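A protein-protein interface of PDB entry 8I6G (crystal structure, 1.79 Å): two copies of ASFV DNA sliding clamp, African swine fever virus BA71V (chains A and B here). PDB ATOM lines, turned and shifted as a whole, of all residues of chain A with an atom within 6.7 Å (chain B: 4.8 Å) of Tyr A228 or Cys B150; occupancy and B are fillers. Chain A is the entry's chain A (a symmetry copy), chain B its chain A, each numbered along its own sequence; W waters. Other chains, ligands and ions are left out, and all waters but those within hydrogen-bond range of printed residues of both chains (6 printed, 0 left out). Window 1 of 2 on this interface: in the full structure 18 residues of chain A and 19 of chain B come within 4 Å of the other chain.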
ATOM      1  N   LYS A 193     -11.384 -20.518 -36.688  1.00  0.00           N
ATOM      2  CA  LYS A 193     -12.124 -19.766 -35.681  1.00  0.00           C
ATOM      3  C   LYS A 193     -12.791 -20.694 -34.656  1.00  0.00           C
ATOM      4  O   LYS A 193     -12.657 -20.528 -33.440  1.00  0.00           O
ATOM      5  CB  LYS A 193     -13.163 -18.887 -36.371  1.00  0.00           C
ATOM      6  CG  LYS A 193     -14.053 -18.115 -35.432  1.00  0.00           C
ATOM      7  CD  LYS A 193     -13.262 -17.045 -34.771  1.00  0.00           C
ATOM      8  CE  LYS A 193     -14.162 -16.144 -33.950  1.00  0.00           C
ATOM      9  NZ  LYS A 193     -13.451 -15.852 -32.701  1.00  0.00           N
ATOM     10  N   THR A 194     -13.492 -21.701 -35.156  1.00  0.00           N
ATOM     11  CA  THR A 194     -14.187 -22.623 -34.279  1.00  0.00           C
ATOM     12  C   THR A 194     -13.216 -23.356 -33.365  1.00  0.00           C
ATOM     13  O   THR A 194     -13.422 -23.422 -32.169  1.00  0.00           O
ATOM     14  CB  THR A 194     -15.002 -23.637 -35.105  1.00  0.00           C
ATOM     15  OG1 THR A 194     -16.153 -22.960 -35.617  1.00  0.00           O
ATOM     16  CG2 THR A 194     -15.450 -24.793 -34.240  1.00  0.00           C
ATOM     17  N   ASP A 197     -11.369 -20.982 -30.831  1.00  0.00           N
ATOM     18  CA  ASP A 197     -12.335 -20.599 -29.785  1.00  0.00           C
ATOM     19  C   ASP A 197     -12.530 -21.713 -28.771  1.00  0.00           C
ATOM     20  O   ASP A 197     -12.538 -21.482 -27.564  1.00  0.00           O
ATOM     21  CB  ASP A 197     -13.698 -20.239 -30.396  1.00  0.00           C
ATOM     22  CG  ASP A 197     -13.743 -18.819 -30.959  1.00  0.00           C
ATOM     23  OD1 ASP A 197     -12.681 -18.153 -30.991  1.00  0.00           O
ATOM     24  OD2 ASP A 197     -14.836 -18.385 -31.403  1.00  0.00           O
ATOM     25  N   LEU A 198     -12.701 -22.934 -29.269  1.00  0.00           N
ATOM     26  CA  LEU A 198     -12.816 -24.082 -28.393  1.00  0.00           C
ATOM     27  C   LEU A 198     -11.533 -24.337 -27.596  1.00  0.00           C
ATOM     28  O   LEU A 198     -11.575 -24.510 -26.372  1.00  0.00           O
ATOM     29  CB  LEU A 198     -13.191 -25.319 -29.206  1.00  0.00           C
ATOM     30  CG  LEU A 198     -14.625 -25.369 -29.750  1.00  0.00           C
ATOM     31  CD1 LEU A 198     -14.782 -26.526 -30.774  1.00  0.00           C
ATOM     32  CD2 LEU A 198     -15.625 -25.509 -28.615  1.00  0.00           C
ATOM     33  N   TYR A 201     -10.455 -23.017 -24.126  1.00  0.00           N
ATOM     34  CA  TYR A 201     -11.058 -23.391 -22.857  1.00  0.00           C
ATOM     35  C   TYR A 201     -11.210 -24.900 -22.666  1.00  0.00           C
ATOM     36  O   TYR A 201     -11.480 -25.345 -21.554  1.00  0.00           O
ATOM     37  CB  TYR A 201     -12.435 -22.715 -22.708  1.00  0.00           C
ATOM     38  CG  TYR A 201     -12.411 -21.201 -22.448  1.00  0.00           C
ATOM     39  CD1 TYR A 201     -12.071 -20.695 -21.199  1.00  0.00           C
ATOM     40  CD2 TYR A 201     -12.789 -20.296 -23.432  1.00  0.00           C
ATOM     41  CE1 TYR A 201     -12.077 -19.323 -20.948  1.00  0.00           C
ATOM     42  CE2 TYR A 201     -12.804 -18.924 -23.196  1.00  0.00           C
ATOM     43  CZ  TYR A 201     -12.445 -18.446 -21.952  1.00  0.00           C
ATOM     44  OH  TYR A 201     -12.470 -17.079 -21.722  1.00  0.00           O
ATOM     45  N   VAL A 205     -14.800 -31.639 -27.134  1.00  0.00           N
ATOM     46  CA  VAL A 205     -16.054 -30.989 -27.486  1.00  0.00           C
ATOM     47  C   VAL A 205     -17.103 -32.031 -27.866  1.00  0.00           C
ATOM     48  O   VAL A 205     -16.780 -33.091 -28.412  1.00  0.00           O
ATOM     49  CB  VAL A 205     -15.866 -29.955 -28.632  1.00  0.00           C
ATOM     50  CG1 VAL A 205     -15.592 -30.638 -29.951  1.00  0.00           C
ATOM     51  CG2 VAL A 205     -17.084 -29.022 -28.734  1.00  0.00           C
ATOM     52  N   LEU A 218     -22.108 -27.532 -31.266  1.00  0.00           N
ATOM     53  CA  LEU A 218     -20.778 -27.853 -30.738  1.00  0.00           C
ATOM     54  C   LEU A 218     -20.732 -27.252 -29.336  1.00  0.00           C
ATOM     55  O   LEU A 218     -20.982 -26.050 -29.176  1.00  0.00           O
ATOM     56  CB  LEU A 218     -19.636 -27.283 -31.617  1.00  0.00           C
ATOM     57  CG  LEU A 218     -19.796 -27.411 -33.138  1.00  0.00           C
ATOM     58  CD1 LEU A 218     -18.637 -26.753 -33.913  1.00  0.00           C
ATOM     59  CD2 LEU A 218     -19.967 -28.871 -33.531  1.00  0.00           C
ATOM     60  N   TYR A 219     -20.474 -28.053 -28.307  1.00  0.00           N
ATOM     61  CA  TYR A 219     -20.513 -27.478 -26.965  1.00  0.00           C
ATOM     62  C   TYR A 219     -19.694 -28.228 -25.920  1.00  0.00           C
ATOM     63  O   TYR A 219     -19.289 -29.371 -26.134  1.00  0.00           O
ATOM     64  CB  TYR A 219     -21.964 -27.362 -26.487  1.00  0.00           C
ATOM     65  CG  TYR A 219     -22.654 -28.673 -26.202  1.00  0.00           C
ATOM     66  CD1 TYR A 219     -23.339 -29.355 -27.202  1.00  0.00           C
ATOM     67  CD2 TYR A 219     -22.657 -29.212 -24.923  1.00  0.00           C
ATOM     68  CE1 TYR A 219     -23.996 -30.565 -26.932  1.00  0.00           C
ATOM     69  CE2 TYR A 219     -23.305 -30.424 -24.645  1.00  0.00           C
ATOM     70  CZ  TYR A 219     -23.971 -31.088 -25.656  1.00  0.00           C
ATOM     71  OH  TYR A 219     -24.635 -32.268 -25.383  1.00  0.00           O
ATOM     72  N   PHE A 220     -19.429 -27.555 -24.798  1.00  0.00           N
ATOM     73  CA  PHE A 220     -18.769 -28.185 -23.657  1.00  0.00           C
ATOM     74  C   PHE A 220     -19.192 -27.483 -22.383  1.00  0.00           C
ATOM     75  O   PHE A 220     -19.713 -26.362 -22.431  1.00  0.00           O
ATOM     76  CB  PHE A 220     -17.223 -28.147 -23.781  1.00  0.00           C
ATOM     77  CG  PHE A 220     -16.631 -26.757 -23.661  1.00  0.00           C
ATOM     78  CD1 PHE A 220     -16.425 -26.166 -22.414  1.00  0.00           C
ATOM     79  CD2 PHE A 220     -16.283 -26.041 -24.799  1.00  0.00           C
ATOM     80  CE1 PHE A 220     -15.897 -24.879 -22.312  1.00  0.00           C
ATOM     81  CE2 PHE A 220     -15.736 -24.766 -24.707  1.00  0.00           C
ATOM     82  CZ  PHE A 220     -15.550 -24.180 -23.458  1.00  0.00           C
ATOM     83  N   GLN A 221     -18.941 -28.133 -21.249  1.00  0.00           N
ATOM     84  CA  GLN A 221     -19.180 -27.540 -19.937  1.00  0.00           C
ATOM     85  C   GLN A 221     -17.991 -27.724 -18.986  1.00  0.00           C
ATOM     86  O   GLN A 221     -17.499 -28.839 -18.806  1.00  0.00           O
ATOM     87  CB  GLN A 221     -20.432 -28.132 -19.292  1.00  0.00           C
ATOM     88  CG  GLN A 221     -20.657 -27.591 -17.886  1.00  0.00           C
ATOM     89  CD  GLN A 221     -21.754 -28.312 -17.118  1.00  0.00           C
ATOM     90  OE1 GLN A 221     -22.084 -29.457 -17.409  1.00  0.00           O
ATOM     91  NE2 GLN A 221     -22.315 -27.635 -16.123  1.00  0.00           N
ATOM     92  N   LYS A 222     -17.528 -26.623 -18.390  1.00  0.00           N
ATOM     93  CA  LYS A 222     -16.530 -26.678 -17.323  1.00  0.00           C
ATOM     94  C   LYS A 222     -17.193 -26.159 -16.053  1.00  0.00           C
ATOM     95  O   LYS A 222     -17.395 -24.956 -15.933  1.00  0.00           O
ATOM     96  CB  LYS A 222     -15.283 -25.832 -17.641  1.00  0.00           C
ATOM     97  CG  LYS A 222     -14.533 -26.169 -18.957  1.00  0.00           C
ATOM     98  CD  LYS A 222     -13.957 -27.582 -18.935  1.00  0.00           C
ATOM     99  CE  LYS A 222     -13.094 -27.856 -20.170  1.00  0.00           C
ATOM    100  NZ  LYS A 222     -13.050 -29.321 -20.473  1.00  0.00           N
ATOM    101  N   ILE A 226     -16.995 -21.964 -16.917  1.00  0.00           N
ATOM    102  CA  ILE A 226     -17.468 -21.540 -18.220  1.00  0.00           C
ATOM    103  C   ILE A 226     -18.059 -22.716 -18.990  1.00  0.00           C
ATOM    104  O   ILE A 226     -17.495 -23.803 -18.973  1.00  0.00           O
ATOM    105  CB  ILE A 226     -16.309 -20.900 -19.047  1.00  0.00           C
ATOM    106  CG1 ILE A 226     -16.781 -20.502 -20.448  1.00  0.00           C
ATOM    107  CG2 ILE A 226     -15.130 -21.858 -19.154  1.00  0.00           C
ATOM    108  CD1 ILE A 226     -15.638 -20.064 -21.383  1.00  0.00           C
ATOM    109  N   SER A 227     -19.208 -22.500 -19.622  1.00  0.00           N
ATOM    110  CA  SER A 227     -19.734 -23.417 -20.626  1.00  0.00           C
ATOM    111  C   SER A 227     -19.846 -22.659 -21.929  1.00  0.00           C
ATOM    112  O   SER A 227     -20.066 -21.459 -21.932  1.00  0.00           O
ATOM    113  CB  SER A 227     -21.101 -23.985 -20.212  1.00  0.00           C
ATOM    114  OG  SER A 227     -20.963 -24.700 -19.002  1.00  0.00           O
ATOM    115  N   TYR A 228     -19.706 -23.352 -23.048  1.00  0.00           N
ATOM    116  CA  TYR A 228     -19.721 -22.692 -24.342  1.00  0.00           C
ATOM    117  C   TYR A 228     -20.534 -23.525 -25.318  1.00  0.00           C
ATOM    118  O   TYR A 228     -20.441 -24.745 -25.292  1.00  0.00           O
ATOM    119  CB  TYR A 228     -18.298 -22.511 -24.855  1.00  0.00           C
ATOM    120  CG  TYR A 228     -18.166 -22.020 -26.280  1.00  0.00           C
ATOM    121  CD1 TYR A 228     -18.402 -20.695 -26.593  1.00  0.00           C
ATOM    122  CD2 TYR A 228     -17.804 -22.887 -27.311  1.00  0.00           C
ATOM    123  CE1 TYR A 228     -18.274 -20.234 -27.881  1.00  0.00           C
ATOM    124  CE2 TYR A 228     -17.684 -22.433 -28.616  1.00  0.00           C
ATOM    125  CZ  TYR A 228     -17.912 -21.090 -28.888  1.00  0.00           C
ATOM    126  OH  TYR A 228     -17.798 -20.596 -30.170  1.00  0.00           O
ATOM    127  N   HIS A 229     -21.292 -22.853 -26.177  1.00  0.00           N
ATOM    128  CA  HIS A 229     -22.202 -23.512 -27.109  1.00  0.00           C
ATOM    129  C   HIS A 229     -22.194 -22.773 -28.429  1.00  0.00           C
ATOM    130  O   HIS A 229     -22.514 -21.578 -28.497  1.00  0.00           O
ATOM    131  CB  HIS A 229     -23.601 -23.552 -26.501  1.00  0.00           C
ATOM    132  CG  HIS A 229     -24.633 -24.207 -27.363  1.00  0.00           C
ATOM    133  ND1 HIS A 229     -25.963 -23.855 -27.304  1.00  0.00           N
ATOM    134  CD2 HIS A 229     -24.538 -25.173 -28.300  1.00  0.00           C
ATOM    135  CE1 HIS A 229     -26.649 -24.603 -28.151  1.00  0.00           C
ATOM    136  NE2 HIS A 229     -25.806 -25.407 -28.778  1.00  0.00           N
ATOM    137  N   GLU A 230     -21.777 -23.483 -29.458  1.00  0.00           N
ATOM    138  CA  GLU A 230     -21.778 -22.999 -30.821  1.00  0.00           C
ATOM    139  C   GLU A 230     -22.927 -23.665 -31.576  1.00  0.00           C
ATOM    140  O   GLU A 230     -22.933 -24.882 -31.719  1.00  0.00           O
ATOM    141  CB  GLU A 230     -20.441 -23.322 -31.491  1.00  0.00           C
ATOM    142  CG  GLU A 230     -19.892 -22.211 -32.301  1.00  0.00           C
ATOM    143  CD  GLU A 230     -18.491 -22.492 -32.808  1.00  0.00           C
ATOM    144  OE1 GLU A 230     -18.374 -23.169 -33.843  1.00  0.00           O
ATOM    145  OE2 GLU A 230     -17.517 -22.022 -32.171  1.00  0.00           O
ATOM    146  N   MET A 231     -23.893 -22.881 -32.041  1.00  0.00           N
ATOM    147  CA  MET A 231     -25.047 -23.453 -32.730  1.00  0.00           C
ATOM    148  C   MET A 231     -25.163 -22.936 -34.157  1.00  0.00           C
ATOM    149  O   MET A 231     -25.127 -21.730 -34.408  1.00  0.00           O
ATOM    150  CB  MET A 231     -26.329 -23.154 -31.959  1.00  0.00           C
ATOM    151  CG  MET A 231     -27.530 -23.879 -32.536  1.00  0.00           C
ATOM    152  SD  MET A 231     -29.034 -23.267 -31.786  1.00  0.00           S
ATOM    153  CE  MET A 231     -28.849 -23.866 -30.156  1.00  0.00           C
ATOM    154  N   TYR A 232     -25.287 -23.867 -35.090  1.00  0.00           N
ATOM    155  CA  TYR A 232     -25.436 -23.570 -36.503  1.00  0.00           C
ATOM    156  C   TYR A 232     -26.888 -23.760 -36.931  1.00  0.00           C
ATOM    157  O   TYR A 232     -27.336 -24.887 -37.146  1.00  0.00           O
ATOM    158  CB  TYR A 232     -24.502 -24.465 -37.325  1.00  0.00           C
ATOM    159  CG  TYR A 232     -23.056 -24.108 -37.057  1.00  0.00           C
ATOM    160  CD1 TYR A 232     -22.374 -24.648 -35.971  1.00  0.00           C
ATOM    161  CD2 TYR A 232     -22.399 -23.190 -37.854  1.00  0.00           C
ATOM    162  CE1 TYR A 232     -21.057 -24.291 -35.706  1.00  0.00           C
ATOM    163  CE2 TYR A 232     -21.082 -22.829 -37.598  1.00  0.00           C
ATOM    164  CZ  TYR A 232     -20.424 -23.393 -36.527  1.00  0.00           C
ATOM    165  OH  TYR A 232     -19.125 -23.033 -36.259  1.00  0.00           O
ATOM    166  N   PHE B 122     -18.053 -11.466 -35.991  1.00  0.00           N
ATOM    167  CA  PHE B 122     -19.148 -11.212 -35.057  1.00  0.00           C
ATOM    168  C   PHE B 122     -19.697  -9.797 -35.245  1.00  0.00           C
ATOM    169  O   PHE B 122     -18.965  -8.826 -35.081  1.00  0.00           O
ATOM    170  CB  PHE B 122     -18.682 -11.388 -33.608  1.00  0.00           C
ATOM    171  CG  PHE B 122     -18.341 -12.805 -33.233  1.00  0.00           C
ATOM    172  CD1 PHE B 122     -18.991 -13.874 -33.829  1.00  0.00           C
ATOM    173  CD2 PHE B 122     -17.379 -13.065 -32.267  1.00  0.00           C
ATOM    174  CE1 PHE B 122     -18.688 -15.181 -33.469  1.00  0.00           C
ATOM    175  CE2 PHE B 122     -17.069 -14.362 -31.901  1.00  0.00           C
ATOM    176  CZ  PHE B 122     -17.722 -15.427 -32.507  1.00  0.00           C
ATOM    177  N   PHE B 139     -23.047 -14.348 -22.462  1.00  0.00           N
ATOM    178  CA  PHE B 139     -22.526 -13.563 -23.580  1.00  0.00           C
ATOM    179  C   PHE B 139     -22.812 -14.293 -24.879  1.00  0.00           C
ATOM    180  O   PHE B 139     -22.388 -15.452 -25.087  1.00  0.00           O
ATOM    181  CB  PHE B 139     -21.017 -13.315 -23.457  1.00  0.00           C
ATOM    182  CG  PHE B 139     -20.628 -12.523 -22.254  1.00  0.00           C
ATOM    183  CD1 PHE B 139     -20.511 -13.134 -21.020  1.00  0.00           C
ATOM    184  CD2 PHE B 139     -20.333 -11.161 -22.366  1.00  0.00           C
ATOM    185  CE1 PHE B 139     -20.151 -12.397 -19.890  1.00  0.00           C
ATOM    186  CE2 PHE B 139     -19.944 -10.423 -21.252  1.00  0.00           C
ATOM    187  CZ  PHE B 139     -19.842 -11.044 -20.017  1.00  0.00           C
ATOM    188  N   ILE B 140     -23.522 -13.631 -25.778  1.00  0.00           N
ATOM    189  CA  ILE B 140     -23.885 -14.282 -27.024  1.00  0.00           C
ATOM    190  C   ILE B 140     -23.342 -13.511 -28.206  1.00  0.00           C
ATOM    191  O   ILE B 140     -23.627 -12.319 -28.365  1.00  0.00           O
ATOM    192  CB  ILE B 140     -25.423 -14.442 -27.162  1.00  0.00           C
ATOM    193  CG1 ILE B 140     -25.989 -15.229 -25.986  1.00  0.00           C
ATOM    194  CG2 ILE B 140     -25.784 -15.146 -28.464  1.00  0.00           C
ATOM    195  CD1 ILE B 140     -26.577 -14.366 -24.915  1.00  0.00           C
ATOM    196  N   PHE B 141     -22.551 -14.201 -29.026  1.00  0.00           N
ATOM    197  CA  PHE B 141     -21.976 -13.612 -30.229  1.00  0.00           C
ATOM    198  C   PHE B 141     -22.585 -14.227 -31.476  1.00  0.00           C
ATOM    199  O   PHE B 141     -22.744 -15.450 -31.559  1.00  0.00           O
ATOM    200  CB  PHE B 141     -20.450 -13.795 -30.239  1.00  0.00           C
ATOM    201  CG  PHE B 141     -19.771 -13.196 -29.035  1.00  0.00           C
ATOM    202  CD1 PHE B 141     -19.496 -11.839 -28.981  1.00  0.00           C
ATOM    203  CD2 PHE B 141     -19.426 -13.985 -27.948  1.00  0.00           C
ATOM    204  CE1 PHE B 141     -18.889 -11.281 -27.861  1.00  0.00           C
ATOM    205  CE2 PHE B 141     -18.808 -13.426 -26.822  1.00  0.00           C
ATOM    206  CZ  PHE B 141     -18.544 -12.073 -26.787  1.00  0.00           C
ATOM    207  N   LYS B 148     -24.515 -18.501 -37.315  1.00  0.00           N
ATOM    208  CA  LYS B 148     -23.813 -19.148 -36.220  1.00  0.00           C
ATOM    209  C   LYS B 148     -23.955 -18.318 -34.962  1.00  0.00           C
ATOM    210  O   LYS B 148     -23.713 -17.107 -34.984  1.00  0.00           O
ATOM    211  CB  LYS B 148     -22.326 -19.331 -36.553  1.00  0.00           C
ATOM    212  CG  LYS B 148     -21.484 -19.757 -35.353  1.00  0.00           C
ATOM    213  CD  LYS B 148     -20.045 -20.085 -35.750  1.00  0.00           C
ATOM    214  CE  LYS B 148     -19.117 -18.920 -35.590  1.00  0.00           C
ATOM    215  NZ  LYS B 148     -17.672 -19.332 -35.642  1.00  0.00           N
ATOM    216  N   GLU B 149     -24.316 -18.973 -33.868  1.00  0.00           N
ATOM    217  CA  GLU B 149     -24.511 -18.304 -32.602  1.00  0.00           C
ATOM    218  C   GLU B 149     -23.628 -18.941 -31.538  1.00  0.00           C
ATOM    219  O   GLU B 149     -23.687 -20.150 -31.302  1.00  0.00           O
ATOM    220  CB  GLU B 149     -25.987 -18.377 -32.225  1.00  0.00           C
ATOM    221  CG  GLU B 149     -26.428 -17.485 -31.135  1.00  0.00           C
ATOM    222  CD  GLU B 149     -27.927 -17.606 -30.938  1.00  0.00           C
ATOM    223  OE1 GLU B 149     -28.352 -18.476 -30.148  1.00  0.00           O
ATOM    224  OE2 GLU B 149     -28.675 -16.861 -31.607  1.00  0.00           O
ATOM    225  N   CYS B 150     -22.793 -18.124 -30.905  1.00  0.00           N
ATOM    226  CA  CYS B 150     -21.847 -18.601 -29.910  1.00  0.00           C
ATOM    227  C   CYS B 150     -22.230 -18.101 -28.532  1.00  0.00           C
ATOM    228  O   CYS B 150     -22.177 -16.881 -28.260  1.00  0.00           O
ATOM    229  CB  CYS B 150     -20.424 -18.129 -30.259  1.00  0.00           C
ATOM    230  SG  CYS B 150     -19.884 -18.669 -31.885  1.00  0.00           S
ATOM    231  N   THR B 151     -22.598 -19.026 -27.653  1.00  0.00           N
ATOM    232  CA  THR B 151     -23.079 -18.657 -26.336  1.00  0.00           C
ATOM    233  C   THR B 151     -22.137 -19.091 -25.216  1.00  0.00           C
ATOM    234  O   THR B 151     -21.848 -20.282 -25.052  1.00  0.00           O
ATOM    235  CB  THR B 151     -24.481 -19.248 -26.092  1.00  0.00           C
ATOM    236  OG1 THR B 151     -25.411 -18.671 -27.018  1.00  0.00           O
ATOM    237  CG2 THR B 151     -24.934 -18.960 -24.699  1.00  0.00           C
ATOM    238  N   TYR B 152     -21.645 -18.104 -24.466  1.00  0.00           N
ATOM    239  CA  TYR B 152     -20.814 -18.345 -23.294  1.00  0.00           C
ATOM    240  C   TYR B 152     -21.643 -18.227 -22.024  1.00  0.00           C
ATOM    241  O   TYR B 152     -22.370 -17.240 -21.830  1.00  0.00           O
ATOM    242  CB  TYR B 152     -19.640 -17.331 -23.227  1.00  0.00           C
ATOM    243  CG  TYR B 152     -18.579 -17.493 -24.290  1.00  0.00           C
ATOM    244  CD1 TYR B 152     -18.757 -16.953 -25.560  1.00  0.00           C
ATOM    245  CD2 TYR B 152     -17.390 -18.148 -24.012  1.00  0.00           C
ATOM    246  CE1 TYR B 152     -17.819 -17.080 -26.512  1.00  0.00           C
ATOM    247  CE2 TYR B 152     -16.409 -18.275 -24.987  1.00  0.00           C
ATOM    248  CZ  TYR B 152     -16.635 -17.733 -26.231  1.00  0.00           C
ATOM    249  OH  TYR B 152     -15.703 -17.878 -27.205  1.00  0.00           O
HETATM  250  O   HOH W   1     -25.516 -20.750 -28.900  1.00  0.00           O
HETATM  251  O   HOH W   2     -16.535 -19.933 -33.166  1.00  0.00           O
HETATM  252  O   HOH W   3     -23.241 -22.283 -23.342  1.00  0.00           O
HETATM  253  O   HOH W   4     -13.048 -18.906 -26.692  1.00  0.00           O
HETATM  254  O   HOH W   5     -17.097 -21.401 -37.706  1.00  0.00           O
HETATM  255  O   HOH W   6     -16.163 -17.185 -29.464  1.00  0.00           O
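Water W6 bridges OH of Tyr B152 (2.4 Å) and OD2 of Asp A197 (2.6 Å).
Water W2 lies within hydrogen-bond range of the side-chain carboxylate (OE2) of Glu A230 (2.5 Å), the side-chain amino group (NZ) of Lys B148 (2.8 Å), the side-chain carboxylate (OD2) of Asp A197 (2.9 Å) and the side-chain hydroxyl (OH) of Tyr A228 (3.3 Å).
Water W4 bridges the backbone carbonyl oxygen of Asp A197 (2.8 Å) and the side-chain hydroxyl of Tyr B152 (2.9 Å).
Water W5 lies within hydrogen-bond range of OG1 of Thr A194 (2.8 Å), OH of Tyr A232 (3.0 Å) and NZ of Lys B148 (3.0 Å).
Water W1 lies within hydrogen-bond range of the side-chain hydroxyl of Thr B151, the backbone carbonyl oxygen of Glu B149 and the backbone carbonyl oxygen of His A229.
Water W3 bridges O of Thr B151 and N of His A229.
Of the 18 printed residues of chain A, 9 touch a printed residue of chain B.
Hydrophobic or aromatic side chains of chain A within 4 Å of the printed part of chain B: Ile A226, Tyr A228, His A229 and Tyr A232.
Hydrophobic or aromatic side chains of chain B within 4 Å of the printed part of chain A: Phe B122 and Tyr B152.
Among the printed residues, 18 pairs touch across the chains.
No position is printed for both chains.
Of the 18 pairs that touch across the chains among the printed residues, none has its exchanged pair printed and touching as well.
The backbone NH (N) of Glu A230 lies within hydrogen-bond range of the backbone carbonyl oxygen (O) of Leu A218.
The side-chain carboxylate (OE1) of Glu A230 lies within hydrogen-bond range of the side-chain hydroxyl (OH) of Tyr A232 (2.5 Å).
The side-chain amino group (NZ) of Lys A193 is in salt-bridge range of the side-chain carboxylate (OD1) of Asp A197 (3.0 Å).
OG1 of Thr A194 is in hydrogen-bond range of OH of Tyr A232 (3.0 Å).
The side-chain carboxylate (OE1) of Glu A230 sits at hydrogen-bond distance from the side-chain hydroxyl (OG1) of Thr A194 (2.9 Å).
The backbone NH (N) of Phe A220 lies within hydrogen-bond range of the backbone carbonyl oxygen (O) of Tyr A228.
Lys A193 touches Phe B122.
Lys B148 touches Lys A193 (NZ to CG, 3.8 Å).
Ile A226 touches Tyr B152 (CD1 to CD2, 3.7 Å).
Thr B151 touches Ser A227.
Ser A227 touches Tyr B152 (O to CA, 3.5 Å).
Tyr B152 touches Tyr A228.
CA of Glu A230 touches O of Glu B149, 3.5 Å away.
Glu A230 touches Cys B150 (CG to SG, 3.6 Å).
Met A231 touches Lys B148 (O to CA, 3.4 Å).
Tyr A232 touches Lys B148 (OH to CD, 3.1 Å).
Of chain A, only Tyr A228 (3.3 Å), His A229 (3.4 Å) and Glu A230 (3.6 Å) come within 4 Å of Cys B150.
Printed residues of chain B within 4 Å of Ile A226: Tyr B152.
Printed residues of chain A within 4 Å of Glu B149: His A229 (3.4 Å), Glu A230 (3.5 Å) and Met A231 (2.8 Å).
The nearest residue of chain A that does not touch Cys B150 is Met A231 (5.0 Å).
The nearest printed residue of chain A that does not touch Thr B151 is Glu A230 (4.9 Å).
O of His A229 sits close to O of Glu B149, at 3.4 Å.
The backbone NH of Thr B151 is in hydrogen-bond range of the backbone carbonyl oxygen of His A229, at 2.7 Å.
The side-chain hydroxyl of Tyr A228 lies within hydrogen-bond range of the side-chain sulfur of Cys B150, at 3.3 Å.
The backbone NH of Met A231 is in hydrogen-bond range of the backbone carbonyl oxygen of Glu B149.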
